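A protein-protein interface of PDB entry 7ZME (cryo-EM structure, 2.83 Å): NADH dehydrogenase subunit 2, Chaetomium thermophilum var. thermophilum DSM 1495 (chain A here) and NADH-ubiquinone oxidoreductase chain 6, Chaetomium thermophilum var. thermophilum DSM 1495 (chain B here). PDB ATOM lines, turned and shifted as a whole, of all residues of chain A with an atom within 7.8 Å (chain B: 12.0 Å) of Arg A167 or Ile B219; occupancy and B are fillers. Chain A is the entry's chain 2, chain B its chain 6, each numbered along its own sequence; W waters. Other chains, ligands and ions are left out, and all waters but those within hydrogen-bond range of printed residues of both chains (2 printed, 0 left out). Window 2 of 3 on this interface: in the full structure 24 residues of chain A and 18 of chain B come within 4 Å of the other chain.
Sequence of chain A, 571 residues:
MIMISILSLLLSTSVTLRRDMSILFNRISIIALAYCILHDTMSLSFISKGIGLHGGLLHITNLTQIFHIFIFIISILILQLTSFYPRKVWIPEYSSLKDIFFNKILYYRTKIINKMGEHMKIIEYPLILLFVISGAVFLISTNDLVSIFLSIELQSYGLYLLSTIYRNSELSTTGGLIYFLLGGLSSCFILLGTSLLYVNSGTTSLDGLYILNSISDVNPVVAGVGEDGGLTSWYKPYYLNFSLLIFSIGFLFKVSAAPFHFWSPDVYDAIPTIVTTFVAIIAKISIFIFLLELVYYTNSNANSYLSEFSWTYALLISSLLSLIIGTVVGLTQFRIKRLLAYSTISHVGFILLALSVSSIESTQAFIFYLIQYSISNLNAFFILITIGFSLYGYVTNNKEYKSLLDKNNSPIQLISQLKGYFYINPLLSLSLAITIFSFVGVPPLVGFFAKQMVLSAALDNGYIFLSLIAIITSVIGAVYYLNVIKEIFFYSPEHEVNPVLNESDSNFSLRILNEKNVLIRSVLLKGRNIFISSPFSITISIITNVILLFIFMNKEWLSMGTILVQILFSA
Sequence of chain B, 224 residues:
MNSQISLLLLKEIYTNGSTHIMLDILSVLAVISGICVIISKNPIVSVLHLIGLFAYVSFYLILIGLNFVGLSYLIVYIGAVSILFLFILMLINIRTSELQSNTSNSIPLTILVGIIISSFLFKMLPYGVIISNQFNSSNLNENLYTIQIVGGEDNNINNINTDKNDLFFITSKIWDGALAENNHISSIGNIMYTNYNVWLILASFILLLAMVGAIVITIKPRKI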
ATOM      1  N   LEU A  17     -20.623 -42.469 -16.070  1.00  0.00           N
ATOM      2  CA  LEU A  17     -20.646 -41.193 -15.323  1.00  0.00           C
ATOM      3  C   LEU A  17     -19.575 -41.353 -14.238  1.00  0.00           C
ATOM      4  O   LEU A  17     -19.560 -40.541 -13.299  1.00  0.00           O
ATOM      5  CB  LEU A  17     -22.048 -40.935 -14.766  1.00  0.00           C
ATOM      6  CG  LEU A  17     -22.832 -39.818 -15.444  1.00  0.00           C
ATOM      7  CD1 LEU A  17     -21.974 -38.573 -15.601  1.00  0.00           C
ATOM      8  CD2 LEU A  17     -23.355 -40.274 -16.792  1.00  0.00           C
ATOM      9  N   GLU A 118      -8.538 -32.340  -9.543  1.00  0.00           N
ATOM     10  CA  GLU A 118      -9.414 -31.859 -10.641  1.00  0.00           C
ATOM     11  C   GLU A 118      -8.911 -32.345 -12.002  1.00  0.00           C
ATOM     12  O   GLU A 118      -9.750 -32.670 -12.846  1.00  0.00           O
ATOM     13  CB  GLU A 118      -9.556 -30.340 -10.572  1.00  0.00           C
ATOM     14  CG  GLU A 118     -10.297 -29.864  -9.337  1.00  0.00           C
ATOM     15  CD  GLU A 118     -11.698 -30.429  -9.184  1.00  0.00           C
ATOM     16  OE1 GLU A 118     -12.141 -31.170 -10.087  1.00  0.00           O
ATOM     17  OE2 GLU A 118     -12.344 -30.131  -8.160  1.00  0.00           O
ATOM     18  N   ILE A 122     -11.985 -34.910 -14.625  1.00  0.00           N
ATOM     19  CA  ILE A 122     -12.789 -34.542 -15.830  1.00  0.00           C
ATOM     20  C   ILE A 122     -12.699 -35.712 -16.802  1.00  0.00           C
ATOM     21  O   ILE A 122     -11.581 -36.069 -17.175  1.00  0.00           O
ATOM     22  CB  ILE A 122     -12.361 -33.188 -16.431  1.00  0.00           C
ATOM     23  CG1 ILE A 122     -12.324 -32.095 -15.362  1.00  0.00           C
ATOM     24  CG2 ILE A 122     -13.248 -32.806 -17.604  1.00  0.00           C
ATOM     25  CD1 ILE A 122     -11.730 -30.799 -15.837  1.00  0.00           C
ATOM     26  N   GLU A 124     -14.330 -36.033 -19.942  1.00  0.00           N
ATOM     27  CA  GLU A 124     -14.400 -35.665 -21.379  1.00  0.00           C
ATOM     28  C   GLU A 124     -13.157 -34.879 -21.776  1.00  0.00           C
ATOM     29  O   GLU A 124     -13.079 -34.480 -22.936  1.00  0.00           O
ATOM     30  CB  GLU A 124     -15.673 -34.857 -21.648  1.00  0.00           C
ATOM     31  CG  GLU A 124     -16.957 -35.565 -21.247  1.00  0.00           C
ATOM     32  CD  GLU A 124     -17.399 -35.457 -19.793  1.00  0.00           C
ATOM     33  OE1 GLU A 124     -18.549 -35.824 -19.506  1.00  0.00           O
ATOM     34  OE2 GLU A 124     -16.603 -35.002 -18.952  1.00  0.00           O
ATOM     35  N   LEU A 161     -13.819 -24.566 -25.141  1.00  0.00           N
ATOM     36  CA  LEU A 161     -14.386 -25.540 -24.223  1.00  0.00           C
ATOM     37  C   LEU A 161     -13.354 -26.112 -23.264  1.00  0.00           C
ATOM     38  O   LEU A 161     -13.716 -26.508 -22.153  1.00  0.00           O
ATOM     39  CB  LEU A 161     -15.044 -26.672 -25.012  1.00  0.00           C
ATOM     40  CG  LEU A 161     -16.308 -26.309 -25.794  1.00  0.00           C
ATOM     41  CD1 LEU A 161     -16.701 -27.454 -26.692  1.00  0.00           C
ATOM     42  CD2 LEU A 161     -17.448 -25.937 -24.865  1.00  0.00           C
ATOM     43  N   LEU A 162     -12.085 -26.172 -23.667  1.00  0.00           N
ATOM     44  CA  LEU A 162     -11.035 -26.572 -22.738  1.00  0.00           C
ATOM     45  C   LEU A 162     -10.755 -25.479 -21.718  1.00  0.00           C
ATOM     46  O   LEU A 162     -10.505 -25.772 -20.543  1.00  0.00           O
ATOM     47  CB  LEU A 162      -9.760 -26.927 -23.499  1.00  0.00           C
ATOM     48  CG  LEU A 162      -9.620 -28.363 -23.996  1.00  0.00           C
ATOM     49  CD1 LEU A 162      -8.225 -28.595 -24.523  1.00  0.00           C
ATOM     50  CD2 LEU A 162      -9.945 -29.353 -22.898  1.00  0.00           C
ATOM     51  N   SER A 163     -10.938 -24.227 -22.113  1.00  0.00           N
ATOM     52  CA  SER A 163     -10.635 -23.107 -21.192  1.00  0.00           C
ATOM     53  C   SER A 163     -11.739 -23.036 -20.129  1.00  0.00           C
ATOM     54  O   SER A 163     -11.432 -22.592 -19.022  1.00  0.00           O
ATOM     55  CB  SER A 163     -10.525 -21.823 -21.956  1.00  0.00           C
ATOM     56  OG  SER A 163      -9.475 -21.887 -22.906  1.00  0.00           O
ATOM     57  N   THR A 164     -12.944 -23.531 -20.420  1.00  0.00           N
ATOM     58  CA  THR A 164     -14.093 -23.472 -19.479  1.00  0.00           C
ATOM     59  C   THR A 164     -14.340 -24.845 -18.854  1.00  0.00           C
ATOM     60  O   THR A 164     -15.305 -24.970 -18.106  1.00  0.00           O
ATOM     61  CB  THR A 164     -15.348 -23.025 -20.244  1.00  0.00           C
ATOM     62  OG1 THR A 164     -14.915 -22.234 -21.351  1.00  0.00           O
ATOM     63  CG2 THR A 164     -16.330 -22.236 -19.407  1.00  0.00           C
ATOM     64  N   ILE A 165     -13.503 -25.830 -19.146  1.00  0.00           N
ATOM     65  CA  ILE A 165     -13.749 -27.227 -18.676  1.00  0.00           C
ATOM     66  C   ILE A 165     -13.732 -27.303 -17.148  1.00  0.00           C
ATOM     67  O   ILE A 165     -14.394 -28.196 -16.599  1.00  0.00           O
ATOM     68  CB  ILE A 165     -12.861 -28.262 -19.400  1.00  0.00           C
ATOM     69  CG1 ILE A 165     -13.613 -29.576 -19.632  1.00  0.00           C
ATOM     70  CG2 ILE A 165     -11.525 -28.476 -18.710  1.00  0.00           C
ATOM     71  CD1 ILE A 165     -12.986 -30.466 -20.672  1.00  0.00           C
ATOM     72  N   TYR A 166     -12.961 -26.448 -16.485  1.00  0.00           N
ATOM     73  CA  TYR A 166     -12.984 -26.378 -15.001  1.00  0.00           C
ATOM     74  C   TYR A 166     -14.158 -25.471 -14.645  1.00  0.00           C
ATOM     75  O   TYR A 166     -13.927 -24.284 -14.408  1.00  0.00           O
ATOM     76  CB  TYR A 166     -11.629 -25.913 -14.472  1.00  0.00           C
ATOM     77  CG  TYR A 166     -10.548 -26.962 -14.467  1.00  0.00           C
ATOM     78  CD1 TYR A 166      -9.995 -27.424 -15.648  1.00  0.00           C
ATOM     79  CD2 TYR A 166     -10.063 -27.477 -13.279  1.00  0.00           C
ATOM     80  CE1 TYR A 166      -8.993 -28.377 -15.651  1.00  0.00           C
ATOM     81  CE2 TYR A 166      -9.061 -28.431 -13.261  1.00  0.00           C
ATOM     82  CZ  TYR A 166      -8.526 -28.880 -14.452  1.00  0.00           C
ATOM     83  OH  TYR A 166      -7.539 -29.816 -14.449  1.00  0.00           O
ATOM     84  N   ARG A 167     -15.372 -26.019 -14.632  1.00  0.00           N
ATOM     85  CA  ARG A 167     -16.633 -25.259 -14.434  1.00  0.00           C
ATOM     86  C   ARG A 167     -16.717 -24.621 -13.054  1.00  0.00           C
ATOM     87  O   ARG A 167     -17.319 -23.559 -12.952  1.00  0.00           O
ATOM     88  CB  ARG A 167     -17.767 -26.261 -14.643  1.00  0.00           C
ATOM     89  CG  ARG A 167     -17.467 -27.627 -14.049  1.00  0.00           C
ATOM     90  CD  ARG A 167     -18.606 -28.557 -14.378  1.00  0.00           C
ATOM     91  NE  ARG A 167     -19.855 -27.951 -13.958  1.00  0.00           N
ATOM     92  CZ  ARG A 167     -21.027 -28.267 -14.476  1.00  0.00           C
ATOM     93  NH1 ARG A 167     -22.127 -27.680 -14.038  1.00  0.00           N
ATOM     94  NH2 ARG A 167     -21.090 -29.164 -15.440  1.00  0.00           N
ATOM     95  N   ASN A 168     -16.157 -25.270 -12.041  1.00  0.00           N
ATOM     96  CA  ASN A 168     -16.249 -24.792 -10.640  1.00  0.00           C
ATOM     97  C   ASN A 168     -15.177 -23.733 -10.388  1.00  0.00           C
ATOM     98  O   ASN A 168     -15.097 -23.251  -9.249  1.00  0.00           O
ATOM     99  CB  ASN A 168     -16.180 -25.983  -9.689  1.00  0.00           C
ATOM    100  CG  ASN A 168     -17.160 -27.075 -10.053  1.00  0.00           C
ATOM    101  OD1 ASN A 168     -18.180 -26.814 -10.682  1.00  0.00           O
ATOM    102  ND2 ASN A 168     -16.862 -28.300  -9.655  1.00  0.00           N
ATOM    103  N   SER A 169     -14.379 -23.400 -11.406  1.00  0.00           N
ATOM    104  CA  SER A 169     -13.358 -22.328 -11.274  1.00  0.00           C
ATOM    105  C   SER A 169     -13.866 -21.021 -11.882  1.00  0.00           C
ATOM    106  O   SER A 169     -14.135 -21.018 -13.087  1.00  0.00           O
ATOM    107  CB  SER A 169     -12.073 -22.743 -11.914  1.00  0.00           C
ATOM    108  OG  SER A 169     -11.171 -21.652 -11.997  1.00  0.00           O
ATOM    109  N   GLU A 170     -13.973 -19.953 -11.084  1.00  0.00           N
ATOM    110  CA  GLU A 170     -14.378 -18.616 -11.605  1.00  0.00           C
ATOM    111  C   GLU A 170     -13.311 -18.078 -12.564  1.00  0.00           C
ATOM    112  O   GLU A 170     -13.685 -17.414 -13.542  1.00  0.00           O
ATOM    113  CB  GLU A 170     -14.718 -17.641 -10.476  1.00  0.00           C
ATOM    114  CG  GLU A 170     -13.546 -17.258  -9.589  1.00  0.00           C
ATOM    115  CD  GLU A 170     -13.308 -18.130  -8.368  1.00  0.00           C
ATOM    116  OE1 GLU A 170     -13.761 -19.293  -8.367  1.00  0.00           O
ATOM    117  OE2 GLU A 170     -12.677 -17.640  -7.412  1.00  0.00           O
ATOM    118  N   LEU A 171     -12.034 -18.326 -12.268  1.00  0.00           N
ATOM    119  CA  LEU A 171     -10.926 -17.842 -13.126  1.00  0.00           C
ATOM    120  C   LEU A 171     -10.992 -18.489 -14.509  1.00  0.00           C
ATOM    121  O   LEU A 171     -10.790 -17.771 -15.497  1.00  0.00           O
ATOM    122  CB  LEU A 171      -9.595 -18.138 -12.436  1.00  0.00           C
ATOM    123  CG  LEU A 171      -9.197 -17.172 -11.325  1.00  0.00           C
ATOM    124  CD1 LEU A 171      -7.774 -17.442 -10.868  1.00  0.00           C
ATOM    125  CD2 LEU A 171      -9.330 -15.747 -11.812  1.00  0.00           C
ATOM    126  N   SER A 172     -11.241 -19.797 -14.566  1.00  0.00           N
ATOM    127  CA  SER A 172     -11.302 -20.517 -15.864  1.00  0.00           C
ATOM    128  C   SER A 172     -12.517 -20.066 -16.674  1.00  0.00           C
ATOM    129  O   SER A 172     -12.399 -19.943 -17.897  1.00  0.00           O
ATOM    130  CB  SER A 172     -11.247 -22.002 -15.684  1.00  0.00           C
ATOM    131  OG  SER A 172     -10.132 -22.358 -14.887  1.00  0.00           O
ATOM    132  N   THR A 173     -13.642 -19.845 -16.006  1.00  0.00           N
ATOM    133  CA  THR A 173     -14.876 -19.430 -16.715  1.00  0.00           C
ATOM    134  C   THR A 173     -14.620 -18.072 -17.356  1.00  0.00           C
ATOM    135  O   THR A 173     -15.153 -17.828 -18.434  1.00  0.00           O
ATOM    136  CB  THR A 173     -16.118 -19.551 -15.823  1.00  0.00           C
ATOM    137  OG1 THR A 173     -15.866 -18.881 -14.591  1.00  0.00           O
ATOM    138  CG2 THR A 173     -16.496 -20.991 -15.558  1.00  0.00           C
ATOM    139  N   ASN A 409      -5.532 -25.362  -9.339  1.00  0.00           N
ATOM    140  CA  ASN A 409      -5.444 -25.264 -10.820  1.00  0.00           C
ATOM    141  C   ASN A 409      -4.134 -24.600 -11.261  1.00  0.00           C
ATOM    142  O   ASN A 409      -3.568 -25.045 -12.265  1.00  0.00           O
ATOM    143  CB  ASN A 409      -6.699 -24.608 -11.395  1.00  0.00           C
ATOM    144  CG  ASN A 409      -7.971 -25.337 -11.024  1.00  0.00           C
ATOM    145  OD1 ASN A 409      -7.952 -26.538 -10.777  1.00  0.00           O
ATOM    146  ND2 ASN A 409      -9.078 -24.617 -10.989  1.00  0.00           N
ATOM    147  N   PHE B  87     -32.658 -17.449 -22.363  1.00  0.00           N
ATOM    148  CA  PHE B  87     -31.423 -17.269 -21.552  1.00  0.00           C
ATOM    149  C   PHE B  87     -31.397 -15.870 -20.931  1.00  0.00           C
ATOM    150  O   PHE B  87     -30.850 -15.730 -19.841  1.00  0.00           O
ATOM    151  CB  PHE B  87     -30.187 -17.642 -22.375  1.00  0.00           C
ATOM    152  CG  PHE B  87     -29.848 -19.110 -22.396  1.00  0.00           C
ATOM    153  CD1 PHE B  87     -30.667 -20.022 -23.038  1.00  0.00           C
ATOM    154  CD2 PHE B  87     -28.696 -19.579 -21.790  1.00  0.00           C
ATOM    155  CE1 PHE B  87     -30.350 -21.369 -23.062  1.00  0.00           C
ATOM    156  CE2 PHE B  87     -28.379 -20.926 -21.819  1.00  0.00           C
ATOM    157  CZ  PHE B  87     -29.206 -21.819 -22.452  1.00  0.00           C
ATOM    158  N   MET B  90     -33.041 -15.933 -17.690  1.00  0.00           N
ATOM    159  CA  MET B  90     -32.327 -16.697 -16.678  1.00  0.00           C
ATOM    160  C   MET B  90     -31.061 -16.006 -16.185  1.00  0.00           C
ATOM    161  O   MET B  90     -30.724 -16.130 -15.004  1.00  0.00           O
ATOM    162  CB  MET B  90     -32.001 -18.085 -17.237  1.00  0.00           C
ATOM    163  CG  MET B  90     -31.300 -19.030 -16.291  1.00  0.00           C
ATOM    164  SD  MET B  90     -31.018 -20.626 -17.079  1.00  0.00           S
ATOM    165  CE  MET B  90     -29.734 -20.223 -18.250  1.00  0.00           C
ATOM    166  N   LEU B  91     -30.398 -15.233 -17.051  1.00  0.00           N
ATOM    167  CA  LEU B  91     -29.078 -14.662 -16.675  1.00  0.00           C
ATOM    168  C   LEU B  91     -29.089 -13.129 -16.614  1.00  0.00           C
ATOM    169  O   LEU B  91     -28.022 -12.569 -16.332  1.00  0.00           O
ATOM    170  CB  LEU B  91     -28.024 -15.148 -17.676  1.00  0.00           C
ATOM    171  CG  LEU B  91     -28.068 -16.622 -18.073  1.00  0.00           C
ATOM    172  CD1 LEU B  91     -27.202 -16.873 -19.297  1.00  0.00           C
ATOM    173  CD2 LEU B  91     -27.631 -17.514 -16.928  1.00  0.00           C
ATOM    174  N   LEU B 209     -19.036 -31.693 -31.184  1.00  0.00           N
ATOM    175  CA  LEU B 209     -18.236 -31.050 -30.121  1.00  0.00           C
ATOM    176  C   LEU B 209     -19.142 -30.072 -29.373  1.00  0.00           C
ATOM    177  O   LEU B 209     -19.041 -30.001 -28.148  1.00  0.00           O
ATOM    178  CB  LEU B 209     -17.038 -30.352 -30.770  1.00  0.00           C
ATOM    179  CG  LEU B 209     -16.263 -29.361 -29.907  1.00  0.00           C
ATOM    180  CD1 LEU B 209     -15.440 -30.083 -28.854  1.00  0.00           C
ATOM    181  CD2 LEU B 209     -15.369 -28.499 -30.777  1.00  0.00           C
ATOM    182  N   ALA B 210     -20.016 -29.364 -30.086  1.00  0.00           N
ATOM    183  CA  ALA B 210     -20.956 -28.434 -29.427  1.00  0.00           C
ATOM    184  C   ALA B 210     -21.950 -29.196 -28.546  1.00  0.00           C
ATOM    185  O   ALA B 210     -22.230 -28.730 -27.441  1.00  0.00           O
ATOM    186  CB  ALA B 210     -21.644 -27.588 -30.450  1.00  0.00           C
ATOM    187  N   MET B 211     -22.457 -30.327 -29.022  1.00  0.00           N
ATOM    188  CA  MET B 211     -23.419 -31.149 -28.242  1.00  0.00           C
ATOM    189  C   MET B 211     -22.747 -31.687 -26.979  1.00  0.00           C
ATOM    190  O   MET B 211     -23.401 -31.696 -25.931  1.00  0.00           O
ATOM    191  CB  MET B 211     -23.932 -32.322 -29.078  1.00  0.00           C
ATOM    192  CG  MET B 211     -24.636 -31.922 -30.350  1.00  0.00           C
ATOM    193  SD  MET B 211     -25.310 -33.380 -31.180  1.00  0.00           S
ATOM    194  CE  MET B 211     -26.421 -33.985 -29.911  1.00  0.00           C
ATOM    195  N   VAL B 212     -21.491 -32.113 -27.080  1.00  0.00           N
ATOM    196  CA  VAL B 212     -20.764 -32.714 -25.923  1.00  0.00           C
ATOM    197  C   VAL B 212     -20.250 -31.602 -25.008  1.00  0.00           C
ATOM    198  O   VAL B 212     -20.431 -31.729 -23.791  1.00  0.00           O
ATOM    199  CB  VAL B 212     -19.626 -33.637 -26.406  1.00  0.00           C
ATOM    200  CG1 VAL B 212     -18.708 -34.074 -25.274  1.00  0.00           C
ATOM    201  CG2 VAL B 212     -20.164 -34.839 -27.163  1.00  0.00           C
ATOM    202  N   GLY B 213     -19.675 -30.546 -25.578  1.00  0.00           N
ATOM    203  CA  GLY B 213     -19.084 -29.459 -24.779  1.00  0.00           C
ATOM    204  C   GLY B 213     -20.098 -28.604 -24.058  1.00  0.00           C
ATOM    205  O   GLY B 213     -19.843 -28.263 -22.900  1.00  0.00           O
ATOM    206  N   ALA B 214     -21.187 -28.225 -24.722  1.00  0.00           N
ATOM    207  CA  ALA B 214     -22.146 -27.310 -24.064  1.00  0.00           C
ATOM    208  C   ALA B 214     -22.733 -28.031 -22.851  1.00  0.00           C
ATOM    209  O   ALA B 214     -22.904 -27.388 -21.814  1.00  0.00           O
ATOM    210  CB  ALA B 214     -23.204 -26.826 -25.027  1.00  0.00           C
ATOM    211  N   ILE B 215     -23.024 -29.319 -23.002  1.00  0.00           N
ATOM    212  CA  ILE B 215     -23.537 -30.140 -21.870  1.00  0.00           C
ATOM    213  C   ILE B 215     -22.463 -30.317 -20.797  1.00  0.00           C
ATOM    214  O   ILE B 215     -22.798 -30.159 -19.627  1.00  0.00           O
ATOM    215  CB  ILE B 215     -24.108 -31.479 -22.381  1.00  0.00           C
ATOM    216  CG1 ILE B 215     -25.575 -31.330 -22.789  1.00  0.00           C
ATOM    217  CG2 ILE B 215     -23.945 -32.579 -21.343  1.00  0.00           C
ATOM    218  CD1 ILE B 215     -25.856 -30.198 -23.754  1.00  0.00           C
ATOM    219  N   VAL B 216     -21.209 -30.563 -21.183  1.00  0.00           N
ATOM    220  CA  VAL B 216     -20.150 -30.862 -20.175  1.00  0.00           C
ATOM    221  C   VAL B 216     -19.971 -29.665 -19.236  1.00  0.00           C
ATOM    222  O   VAL B 216     -19.793 -29.903 -18.032  1.00  0.00           O
ATOM    223  CB  VAL B 216     -18.821 -31.359 -20.791  1.00  0.00           C
ATOM    224  CG1 VAL B 216     -17.991 -30.252 -21.412  1.00  0.00           C
ATOM    225  CG2 VAL B 216     -17.982 -32.088 -19.759  1.00  0.00           C
ATOM    226  N   ILE B 217     -20.044 -28.438 -19.754  1.00  0.00           N
ATOM    227  CA  ILE B 217     -19.754 -27.241 -18.913  1.00  0.00           C
ATOM    228  C   ILE B 217     -20.973 -26.801 -18.110  1.00  0.00           C
ATOM    229  O   ILE B 217     -20.794 -25.959 -17.232  1.00  0.00           O
ATOM    230  CB  ILE B 217     -19.188 -26.095 -19.768  1.00  0.00           C
ATOM    231  CG1 ILE B 217     -20.148 -25.690 -20.887  1.00  0.00           C
ATOM    232  CG2 ILE B 217     -17.813 -26.458 -20.305  1.00  0.00           C
ATOM    233  CD1 ILE B 217     -19.528 -24.785 -21.917  1.00  0.00           C
ATOM    234  N   THR B 218     -22.162 -27.315 -18.419  1.00  0.00           N
ATOM    235  CA  THR B 218     -23.390 -26.830 -17.746  1.00  0.00           C
ATOM    236  C   THR B 218     -24.127 -27.962 -17.031  1.00  0.00           C
ATOM    237  O   THR B 218     -25.113 -27.653 -16.349  1.00  0.00           O
ATOM    238  CB  THR B 218     -24.329 -26.176 -18.764  1.00  0.00           C
ATOM    239  OG1 THR B 218     -24.741 -27.175 -19.694  1.00  0.00           O
ATOM    240  CG2 THR B 218     -23.705 -25.009 -19.496  1.00  0.00           C
ATOM    241  N   ILE B 219     -23.682 -29.209 -17.179  1.00  0.00           N
ATOM    242  CA  ILE B 219     -24.444 -30.359 -16.609  1.00  0.00           C
ATOM    243  C   ILE B 219     -24.465 -30.295 -15.082  1.00  0.00           C
ATOM    244  O   ILE B 219     -23.440 -29.985 -14.484  1.00  0.00           O
ATOM    245  CB  ILE B 219     -23.924 -31.714 -17.143  1.00  0.00           C
ATOM    246  CG1 ILE B 219     -24.867 -32.872 -16.804  1.00  0.00           C
ATOM    247  CG2 ILE B 219     -22.500 -31.997 -16.694  1.00  0.00           C
ATOM    248  CD1 ILE B 219     -26.271 -32.680 -17.316  1.00  0.00           C
ATOM    249  N   LYS B 220     -25.595 -30.622 -14.469  1.00  0.00           N
ATOM    250  CA  LYS B 220     -25.630 -30.686 -12.990  1.00  0.00           C
ATOM    251  C   LYS B 220     -24.844 -31.929 -12.525  1.00  0.00           C
ATOM    252  O   LYS B 220     -25.019 -32.980 -13.167  1.00  0.00           O
ATOM    253  CB  LYS B 220     -27.074 -30.709 -12.481  1.00  0.00           C
ATOM    254  CG  LYS B 220     -27.858 -29.422 -12.701  1.00  0.00           C
ATOM    255  CD  LYS B 220     -29.276 -29.489 -12.178  1.00  0.00           C
ATOM    256  CE  LYS B 220     -30.015 -28.175 -12.303  1.00  0.00           C
ATOM    257  NZ  LYS B 220     -29.353 -27.097 -11.532  1.00  0.00           N
ATOM    258  N   PRO B 221     -23.999 -31.898 -11.461  1.00  0.00           N
ATOM    259  CA  PRO B 221     -23.239 -33.093 -11.075  1.00  0.00           C
ATOM    260  C   PRO B 221     -24.151 -34.204 -10.581  1.00  0.00           C
ATOM    261  O   PRO B 221     -25.216 -33.954 -10.010  1.00  0.00           O
ATOM    262  CB  PRO B 221     -22.321 -32.584  -9.959  1.00  0.00           C
ATOM    263  CG  PRO B 221     -23.038 -31.405  -9.396  1.00  0.00           C
ATOM    264  CD  PRO B 221     -23.752 -30.765 -10.552  1.00  0.00           C
ATOM    265  N   ARG B 222     -23.722 -35.440 -10.809  1.00  0.00           N
ATOM    266  CA  ARG B 222     -24.490 -36.609 -10.396  1.00  0.00           C
ATOM    267  C   ARG B 222     -23.567 -37.746  -9.970  1.00  0.00           C
ATOM    268  O   ARG B 222     -22.742 -38.217 -10.754  1.00  0.00           O
ATOM    269  CB  ARG B 222     -25.409 -37.072 -11.527  1.00  0.00           C
HETATM  270  O   HOH W   1     -21.291 -24.708 -15.069  1.00  0.00           O
HETATM  271  O   HOH W   2     -16.793 -29.447 -17.103  1.00  0.00           O
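Water W1 lies within hydrogen-bond range of O of Ile B217 and NH1 of Arg A167.
Water W2 bridges the backbone carbonyl oxygen (O) of Ile A165 and the backbone carbonyl oxygen (O) of Val B216.
Of chain B, only Val B216 (3.0 Å), Ile B217 (3.6 Å), Thr B218 (3.6 Å) and Ile B219 (2.7 Å) come within 4 Å of Arg A167.
Printed residues of chain A within 4 Å of Ile B219: Arg A167.
Ile A165 touches none of the printed residues of chain B.
No residue of chain B comes within 4 Å of Ser A169.
Printed residues of chain A within 4 Å of Gly B213: Leu A161.
Printed residues of chain A within 4 Å of Thr B218: Arg A167.
The nearest residue of chain B that does not touch Arg A167 is Lys B220 (4.6 Å).
The nearest residue of chain A that does not touch Ile B219 is Glu A124 (6.2 Å).
Of the 17 printed residues of chain B, 6 touch a printed residue of chain A.
Printed residues of chain B that touch a printed residue of chain A: Leu B209, Gly B213, Val B216, Ile B217, Thr B218 and Ile B219.
Hydrophobic or aromatic side chains of chain B that line the printed part of chain A: Leu B209, Val B216, Ile B217 and Ile B219.
Of the 18 printed residues of chain A, 4 touch a printed residue of chain B.
Hydrophobic or aromatic side chains of chain A within 4 Å of the printed part of chain B: Leu A161.
Among the printed residues, no Asp or Glu carboxylate lies within 4 Å of a Lys or Arg side-chain nitrogen of the other chain.
Among the printed residues, merely in contact across the chains: Glu A124 with Val B216 (3.3 Å), Arg A167 with Ile B217 (3.6 Å), Arg A167 with Thr B218 (3.6 Å), Leu A161 with Leu B209 (3.6 Å), Thr A164 with Ile B217 (3.7 Å), Leu A161 with Gly B213 (3.7 Å) and Leu A161 with Ile B217 (3.8 Å).
The guanidinium group (NH2) of Arg A167 sits at hydrogen-bond distance from the backbone carbonyl oxygen (O) of Val B216 (3.0 Å).
O of Ile B219 is in hydrogen-bond range of NH2 of Arg A167, 2.7 Å away.
The backbone carbonyl oxygen of Ala B214 lies within hydrogen-bond range of the side-chain hydroxyl of Thr B218, 2.8 Å away.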
